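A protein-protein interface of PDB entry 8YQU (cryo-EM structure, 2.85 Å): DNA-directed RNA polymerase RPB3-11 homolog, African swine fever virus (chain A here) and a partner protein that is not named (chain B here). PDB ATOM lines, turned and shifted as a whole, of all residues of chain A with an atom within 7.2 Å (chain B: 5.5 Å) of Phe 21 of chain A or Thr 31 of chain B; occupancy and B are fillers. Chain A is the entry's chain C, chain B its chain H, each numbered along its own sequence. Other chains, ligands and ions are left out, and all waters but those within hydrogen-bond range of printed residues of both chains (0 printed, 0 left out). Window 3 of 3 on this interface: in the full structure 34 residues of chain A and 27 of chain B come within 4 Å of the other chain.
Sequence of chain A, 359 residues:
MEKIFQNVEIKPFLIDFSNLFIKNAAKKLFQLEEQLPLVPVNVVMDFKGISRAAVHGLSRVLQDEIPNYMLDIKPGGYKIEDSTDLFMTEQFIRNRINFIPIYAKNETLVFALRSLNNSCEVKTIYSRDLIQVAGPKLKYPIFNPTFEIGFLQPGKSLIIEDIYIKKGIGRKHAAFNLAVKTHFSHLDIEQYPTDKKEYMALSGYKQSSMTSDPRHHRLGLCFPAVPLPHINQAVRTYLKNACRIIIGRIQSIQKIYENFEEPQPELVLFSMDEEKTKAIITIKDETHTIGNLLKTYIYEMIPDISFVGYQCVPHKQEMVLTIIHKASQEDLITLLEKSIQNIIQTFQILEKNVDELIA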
ATOM      1  N   PHE A  17     -16.937 -17.979  17.797  1.00  0.00           N
ATOM      2  CA  PHE A  17     -17.209 -17.716  19.203  1.00  0.00           C
ATOM      3  C   PHE A  17     -18.311 -18.600  19.768  1.00  0.00           C
ATOM      4  O   PHE A  17     -18.662 -18.454  20.944  1.00  0.00           O
ATOM      5  CB  PHE A  17     -17.567 -16.242  19.408  1.00  0.00           C
ATOM      6  CG  PHE A  17     -16.381 -15.324  19.379  1.00  0.00           C
ATOM      7  CD1 PHE A  17     -15.514 -15.258  20.457  1.00  0.00           C
ATOM      8  CD2 PHE A  17     -16.127 -14.529  18.275  1.00  0.00           C
ATOM      9  CE1 PHE A  17     -14.420 -14.416  20.435  1.00  0.00           C
ATOM     10  CE2 PHE A  17     -15.033 -13.685  18.247  1.00  0.00           C
ATOM     11  CZ  PHE A  17     -14.179 -13.629  19.329  1.00  0.00           C
ATOM     12  N   SER A  18     -18.869 -19.507  18.963  1.00  0.00           N
ATOM     13  CA  SER A  18     -19.801 -20.493  19.492  1.00  0.00           C
ATOM     14  C   SER A  18     -19.100 -21.525  20.366  1.00  0.00           C
ATOM     15  O   SER A  18     -19.766 -22.212  21.147  1.00  0.00           O
ATOM     16  CB  SER A  18     -20.537 -21.192  18.349  1.00  0.00           C
ATOM     17  OG  SER A  18     -21.308 -20.269  17.599  1.00  0.00           O
ATOM     18  N   ASN A  19     -17.781 -21.646  20.249  1.00  0.00           N
ATOM     19  CA  ASN A  19     -17.011 -22.563  21.081  1.00  0.00           C
ATOM     20  C   ASN A  19     -16.755 -21.915  22.435  1.00  0.00           C
ATOM     21  O   ASN A  19     -16.187 -20.820  22.508  1.00  0.00           O
ATOM     22  CB  ASN A  19     -15.697 -22.926  20.393  1.00  0.00           C
ATOM     23  CG  ASN A  19     -15.099 -24.212  20.920  1.00  0.00           C
ATOM     24  OD1 ASN A  19     -15.708 -24.905  21.734  1.00  0.00           O
ATOM     25  ND2 ASN A  19     -13.901 -24.541  20.454  1.00  0.00           N
ATOM     26  N   LEU A  20     -17.176 -22.590  23.508  1.00  0.00           N
ATOM     27  CA  LEU A  20     -17.072 -22.005  24.842  1.00  0.00           C
ATOM     28  C   LEU A  20     -15.619 -21.824  25.266  1.00  0.00           C
ATOM     29  O   LEU A  20     -15.278 -20.824  25.907  1.00  0.00           O
ATOM     30  CB  LEU A  20     -17.822 -22.866  25.860  1.00  0.00           C
ATOM     31  CG  LEU A  20     -19.334 -22.668  26.018  1.00  0.00           C
ATOM     32  CD1 LEU A  20     -19.637 -21.265  26.527  1.00  0.00           C
ATOM     33  CD2 LEU A  20     -20.101 -22.958  24.733  1.00  0.00           C
ATOM     34  N   PHE A  21     -14.753 -22.781  24.928  1.00  0.00           N
ATOM     35  CA  PHE A  21     -13.355 -22.689  25.337  1.00  0.00           C
ATOM     36  C   PHE A  21     -12.679 -21.475  24.712  1.00  0.00           C
ATOM     37  O   PHE A  21     -12.035 -20.680  25.409  1.00  0.00           O
ATOM     38  CB  PHE A  21     -12.615 -23.973  24.959  1.00  0.00           C
ATOM     39  CG  PHE A  21     -13.107 -25.191  25.684  1.00  0.00           C
ATOM     40  CD1 PHE A  21     -12.799 -25.391  27.017  1.00  0.00           C
ATOM     41  CD2 PHE A  21     -13.879 -26.138  25.030  1.00  0.00           C
ATOM     42  CE1 PHE A  21     -13.250 -26.511  27.687  1.00  0.00           C
ATOM     43  CE2 PHE A  21     -14.333 -27.260  25.694  1.00  0.00           C
ATOM     44  CZ  PHE A  21     -14.019 -27.447  27.024  1.00  0.00           C
ATOM     45  N   ILE A  22     -12.821 -21.314  23.395  1.00  0.00           N
ATOM     46  CA  ILE A  22     -12.216 -20.177  22.707  1.00  0.00           C
ATOM     47  C   ILE A  22     -12.824 -18.872  23.198  1.00  0.00           C
ATOM     48  O   ILE A  22     -12.116 -17.882  23.415  1.00  0.00           O
ATOM     49  CB  ILE A  22     -12.364 -20.334  21.182  1.00  0.00           C
ATOM     50  CG1 ILE A  22     -11.687 -21.622  20.715  1.00  0.00           C
ATOM     51  CG2 ILE A  22     -11.781 -19.131  20.461  1.00  0.00           C
ATOM     52  CD1 ILE A  22     -10.224 -21.699  21.077  1.00  0.00           C
ATOM     53  N   LYS A  23     -14.148 -18.848  23.372  1.00  0.00           N
ATOM     54  CA  LYS A  23     -14.819 -17.649  23.860  1.00  0.00           C
ATOM     55  C   LYS A  23     -14.259 -17.214  25.208  1.00  0.00           C
ATOM     56  O   LYS A  23     -13.866 -16.056  25.386  1.00  0.00           O
ATOM     57  CB  LYS A  23     -16.324 -17.905  23.958  1.00  0.00           C
ATOM     58  CG  LYS A  23     -17.140 -16.716  24.427  1.00  0.00           C
ATOM     59  CD  LYS A  23     -18.622 -17.057  24.454  1.00  0.00           C
ATOM     60  CE  LYS A  23     -19.443 -15.925  25.045  1.00  0.00           C
ATOM     61  NZ  LYS A  23     -19.484 -14.739  24.148  1.00  0.00           N
ATOM     62  N   ASN A  24     -14.198 -18.143  26.166  1.00  0.00           N
ATOM     63  CA  ASN A  24     -13.706 -17.806  27.497  1.00  0.00           C
ATOM     64  C   ASN A  24     -12.240 -17.396  27.460  1.00  0.00           C
ATOM     65  O   ASN A  24     -11.849 -16.409  28.097  1.00  0.00           O
ATOM     66  CB  ASN A  24     -13.909 -18.988  28.444  1.00  0.00           C
ATOM     67  CG  ASN A  24     -15.372 -19.265  28.723  1.00  0.00           C
ATOM     68  OD1 ASN A  24     -16.176 -18.344  28.855  1.00  0.00           O
ATOM     69  ND2 ASN A  24     -15.724 -20.542  28.815  1.00  0.00           N
ATOM     70  N   ALA A  25     -11.414 -18.136  26.715  1.00  0.00           N
ATOM     71  CA  ALA A  25      -9.990 -17.823  26.662  1.00  0.00           C
ATOM     72  C   ALA A  25      -9.755 -16.433  26.089  1.00  0.00           C
ATOM     73  O   ALA A  25      -9.002 -15.635  26.659  1.00  0.00           O
ATOM     74  CB  ALA A  25      -9.252 -18.878  25.839  1.00  0.00           C
ATOM     75  N   ALA A  26     -10.406 -16.117  24.965  1.00  0.00           N
ATOM     76  CA  ALA A  26     -10.234 -14.803  24.359  1.00  0.00           C
ATOM     77  C   ALA A  26     -10.764 -13.701  25.264  1.00  0.00           C
ATOM     78  O   ALA A  26     -10.111 -12.665  25.442  1.00  0.00           O
ATOM     79  CB  ALA A  26     -10.928 -14.759  22.998  1.00  0.00           C
ATOM     80  N   LYS A  27     -11.939 -13.914  25.865  1.00  0.00           N
ATOM     81  CA  LYS A  27     -12.549 -12.874  26.684  1.00  0.00           C
ATOM     82  C   LYS A  27     -11.750 -12.608  27.952  1.00  0.00           C
ATOM     83  O   LYS A  27     -11.775 -11.487  28.468  1.00  0.00           O
ATOM     84  CB  LYS A  27     -13.988 -13.258  27.030  1.00  0.00           C
ATOM     85  CG  LYS A  27     -14.810 -12.131  27.632  1.00  0.00           C
ATOM     86  CD  LYS A  27     -14.994 -12.314  29.129  1.00  0.00           C
ATOM     87  CE  LYS A  27     -16.000 -13.411  29.432  1.00  0.00           C
ATOM     88  NZ  LYS A  27     -16.209 -13.586  30.896  1.00  0.00           N
ATOM     89  N   ALA B  24      -7.102 -21.882  26.215  1.00  0.00           N
ATOM     90  CA  ALA B  24      -8.288 -22.700  25.998  1.00  0.00           C
ATOM     91  C   ALA B  24      -7.951 -24.182  26.078  1.00  0.00           C
ATOM     92  O   ALA B  24      -8.630 -24.949  26.774  1.00  0.00           O
ATOM     93  CB  ALA B  24      -8.917 -22.364  24.645  1.00  0.00           C
ATOM     94  N   THR B  26      -5.869 -25.782  27.731  1.00  0.00           N
ATOM     95  CA  THR B  26      -5.723 -26.246  29.104  1.00  0.00           C
ATOM     96  C   THR B  26      -7.060 -26.700  29.675  1.00  0.00           C
ATOM     97  O   THR B  26      -7.177 -27.829  30.169  1.00  0.00           O
ATOM     98  CB  THR B  26      -5.107 -25.147  29.968  1.00  0.00           C
ATOM     99  OG1 THR B  26      -3.820 -24.796  29.446  1.00  0.00           O
ATOM    100  CG2 THR B  26      -4.940 -25.633  31.393  1.00  0.00           C
ATOM    101  N   GLU B  27      -8.099 -25.862  29.567  1.00  0.00           N
ATOM    102  CA  GLU B  27      -9.388 -26.264  30.127  1.00  0.00           C
ATOM    103  C   GLU B  27      -9.889 -27.533  29.459  1.00  0.00           C
ATOM    104  O   GLU B  27     -10.418 -28.431  30.127  1.00  0.00           O
ATOM    105  CB  GLU B  27     -10.434 -25.151  30.015  1.00  0.00           C
ATOM    106  CG  GLU B  27     -10.184 -23.949  30.908  1.00  0.00           C
ATOM    107  CD  GLU B  27      -9.262 -22.946  30.282  1.00  0.00           C
ATOM    108  OE1 GLU B  27      -8.892 -23.156  29.115  1.00  0.00           O
ATOM    109  OE2 GLU B  27      -8.903 -21.954  30.952  1.00  0.00           O
ATOM    110  N   TYR B  28      -9.695 -27.646  28.142  1.00  0.00           N
ATOM    111  CA  TYR B  28     -10.109 -28.865  27.462  1.00  0.00           C
ATOM    112  C   TYR B  28      -9.416 -30.072  28.074  1.00  0.00           C
ATOM    113  O   TYR B  28     -10.060 -31.086  28.368  1.00  0.00           O
ATOM    114  CB  TYR B  28      -9.814 -28.769  25.966  1.00  0.00           C
ATOM    115  CG  TYR B  28     -10.214 -30.002  25.189  1.00  0.00           C
ATOM    116  CD1 TYR B  28     -11.548 -30.265  24.914  1.00  0.00           C
ATOM    117  CD2 TYR B  28      -9.261 -30.901  24.731  1.00  0.00           C
ATOM    118  CE1 TYR B  28     -11.924 -31.387  24.206  1.00  0.00           C
ATOM    119  CE2 TYR B  28      -9.629 -32.028  24.022  1.00  0.00           C
ATOM    120  CZ  TYR B  28     -10.960 -32.265  23.762  1.00  0.00           C
ATOM    121  OH  TYR B  28     -11.331 -33.386  23.055  1.00  0.00           O
ATOM    122  N   ILE B  29      -8.112 -29.953  28.333  1.00  0.00           N
ATOM    123  CA  ILE B  29      -7.394 -31.035  28.997  1.00  0.00           C
ATOM    124  C   ILE B  29      -7.981 -31.279  30.379  1.00  0.00           C
ATOM    125  O   ILE B  29      -8.203 -32.430  30.780  1.00  0.00           O
ATOM    126  CB  ILE B  29      -5.887 -30.722  29.056  1.00  0.00           C
ATOM    127  CG1 ILE B  29      -5.239 -31.021  27.704  1.00  0.00           C
ATOM    128  CG2 ILE B  29      -5.213 -31.523  30.156  1.00  0.00           C
ATOM    129  CD1 ILE B  29      -3.773 -30.674  27.642  1.00  0.00           C
ATOM    130  N   LYS B  30      -8.280 -30.203  31.115  1.00  0.00           N
ATOM    131  CA  LYS B  30      -8.904 -30.362  32.423  1.00  0.00           C
ATOM    132  C   LYS B  30     -10.238 -31.084  32.319  1.00  0.00           C
ATOM    133  O   LYS B  30     -10.650 -31.766  33.264  1.00  0.00           O
ATOM    134  CB  LYS B  30      -9.092 -29.002  33.096  1.00  0.00           C
ATOM    135  CG  LYS B  30      -7.817 -28.391  33.650  1.00  0.00           C
ATOM    136  CD  LYS B  30      -8.119 -27.109  34.410  1.00  0.00           C
ATOM    137  CE  LYS B  30      -6.975 -26.118  34.310  1.00  0.00           C
ATOM    138  NZ  LYS B  30      -7.451 -24.709  34.383  1.00  0.00           N
ATOM    139  N   THR B  31     -10.927 -30.948  31.184  1.00  0.00           N
ATOM    140  CA  THR B  31     -12.176 -31.676  31.002  1.00  0.00           C
ATOM    141  C   THR B  31     -11.918 -33.163  30.805  1.00  0.00           C
ATOM    142  O   THR B  31     -12.682 -34.005  31.294  1.00  0.00           O
ATOM    143  CB  THR B  31     -12.951 -31.095  29.818  1.00  0.00           C
ATOM    144  OG1 THR B  31     -13.273 -29.725  30.086  1.00  0.00           O
ATOM    145  CG2 THR B  31     -14.239 -31.868  29.586  1.00  0.00           C
ATOM    146  N   LYS B  32     -10.837 -33.508  30.109  1.00  0.00           N
ATOM    147  CA  LYS B  32     -10.551 -34.886  29.743  1.00  0.00           C
ATOM    148  C   LYS B  32      -9.466 -35.529  30.597  1.00  0.00           C
ATOM    149  O   LYS B  32      -9.149 -36.702  30.380  1.00  0.00           O
ATOM    150  CB  LYS B  32     -10.143 -34.961  28.267  1.00  0.00           C
ATOM    151  CG  LYS B  32     -11.231 -34.541  27.295  1.00  0.00           C
ATOM    152  CD  LYS B  32     -12.311 -35.601  27.177  1.00  0.00           C
ATOM    153  CE  LYS B  32     -13.337 -35.226  26.121  1.00  0.00           C
ATOM    154  NZ  LYS B  32     -14.222 -34.118  26.575  1.00  0.00           N
ATOM    155  N   MET B  33      -8.885 -34.799  31.551  1.00  0.00           N
ATOM    156  CA  MET B  33      -7.730 -35.311  32.279  1.00  0.00           C
ATOM    157  C   MET B  33      -8.063 -36.570  33.069  1.00  0.00           C
ATOM    158  O   MET B  33      -7.635 -37.668  32.699  1.00  0.00           O
ATOM    159  CB  MET B  33      -7.195 -34.222  33.216  1.00  0.00           C
ATOM    160  CG  MET B  33      -5.971 -34.603  34.018  1.00  0.00           C
ATOM    161  SD  MET B  33      -5.392 -33.239  35.044  1.00  0.00           S
ATOM    162  CE  MET B  33      -6.679 -33.177  36.286  1.00  0.00           C
ATOM    163  N   GLY B  34      -8.819 -36.429  34.154  1.00  0.00           N
ATOM    164  CA  GLY B  34      -9.460 -37.563  34.788  1.00  0.00           C
ATOM    165  C   GLY B  34      -8.587 -38.254  35.814  1.00  0.00           C
ATOM    166  O   GLY B  34      -7.732 -39.061  35.437  1.00  0.00           O
ATOM    167  N   LEU B  54     -11.129 -27.311  18.250  1.00  0.00           N
ATOM    168  CA  LEU B  54     -10.639 -26.074  18.851  1.00  0.00           C
ATOM    169  C   LEU B  54      -9.912 -25.217  17.820  1.00  0.00           C
ATOM    170  O   LEU B  54     -10.181 -24.016  17.684  1.00  0.00           O
ATOM    171  CB  LEU B  54      -9.723 -26.406  20.028  1.00  0.00           C
ATOM    172  CG  LEU B  54      -9.584 -25.377  21.145  1.00  0.00           C
ATOM    173  CD1 LEU B  54     -10.895 -25.241  21.895  1.00  0.00           C
ATOM    174  CD2 LEU B  54      -8.469 -25.784  22.089  1.00  0.00           C
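Of chain B, only Ala 24 (3.6 Å), Glu 27 (3.8 Å), Tyr 28 (3.8 Å), Thr 31 (3.9 Å) and Leu 54 (3.7 Å) come within 4 Å of Phe 21 of chain A.
Asn 24 of chain A touches none of the printed residues of chain B.
Printed residues of chain A within 4 Å of Ala 24 of chain B: Phe 21 (3.6 Å), Ile 22 (3.9 Å) and Ala 25 (3.7 Å).
Thr 26 of chain B touches none of the printed residues of chain A.
Printed residues of chain A within 4 Å of Thr 31 of chain B: Phe 21.
Of the printed residues of chain A, Leu 54 of chain B touches Asn 19, Phe 21 and Ile 22.
The nearest printed residue of chain B that does not touch Phe 21 of chain A is Ile 29 of chain B (6.2 Å).
O of Glu 27 of chain B sits at hydrogen-bond distance from OG1 of Thr 31 of chain B (3.1 Å).
Among the printed residues, merely in contact across the chains: Asn 19 of chain A with Leu 54 of chain B, Phe 21 of chain A with Ala 24 of chain B, Ile 22 of chain A with Leu 54 of chain B, Ala 25 of chain A with Ala 24 of chain B, Phe 21 of chain A with Leu 54 of chain B, Phe 21 of chain A with Tyr 28 of chain B, Phe 21 of chain A with Glu 27 of chain B, Ile 22 of chain A with Ala 24 of chain B and Phe 21 of chain A with Thr 31 of chain B.
Hydrophobic or aromatic side chains of chain B within 4 Å of the printed part of chain A: Ala 24 and Leu 54.
Of the 11 printed residues of chain A, 4 touch a printed residue of chain B.
Hydrophobic or aromatic side chains of chain A that line the printed part of chain B: Phe 21, Ile 22 and Ala 25.
Among the printed residues, no Asp or Glu carboxylate lies within 4 Å of a Lys or Arg side-chain nitrogen of the other chain.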
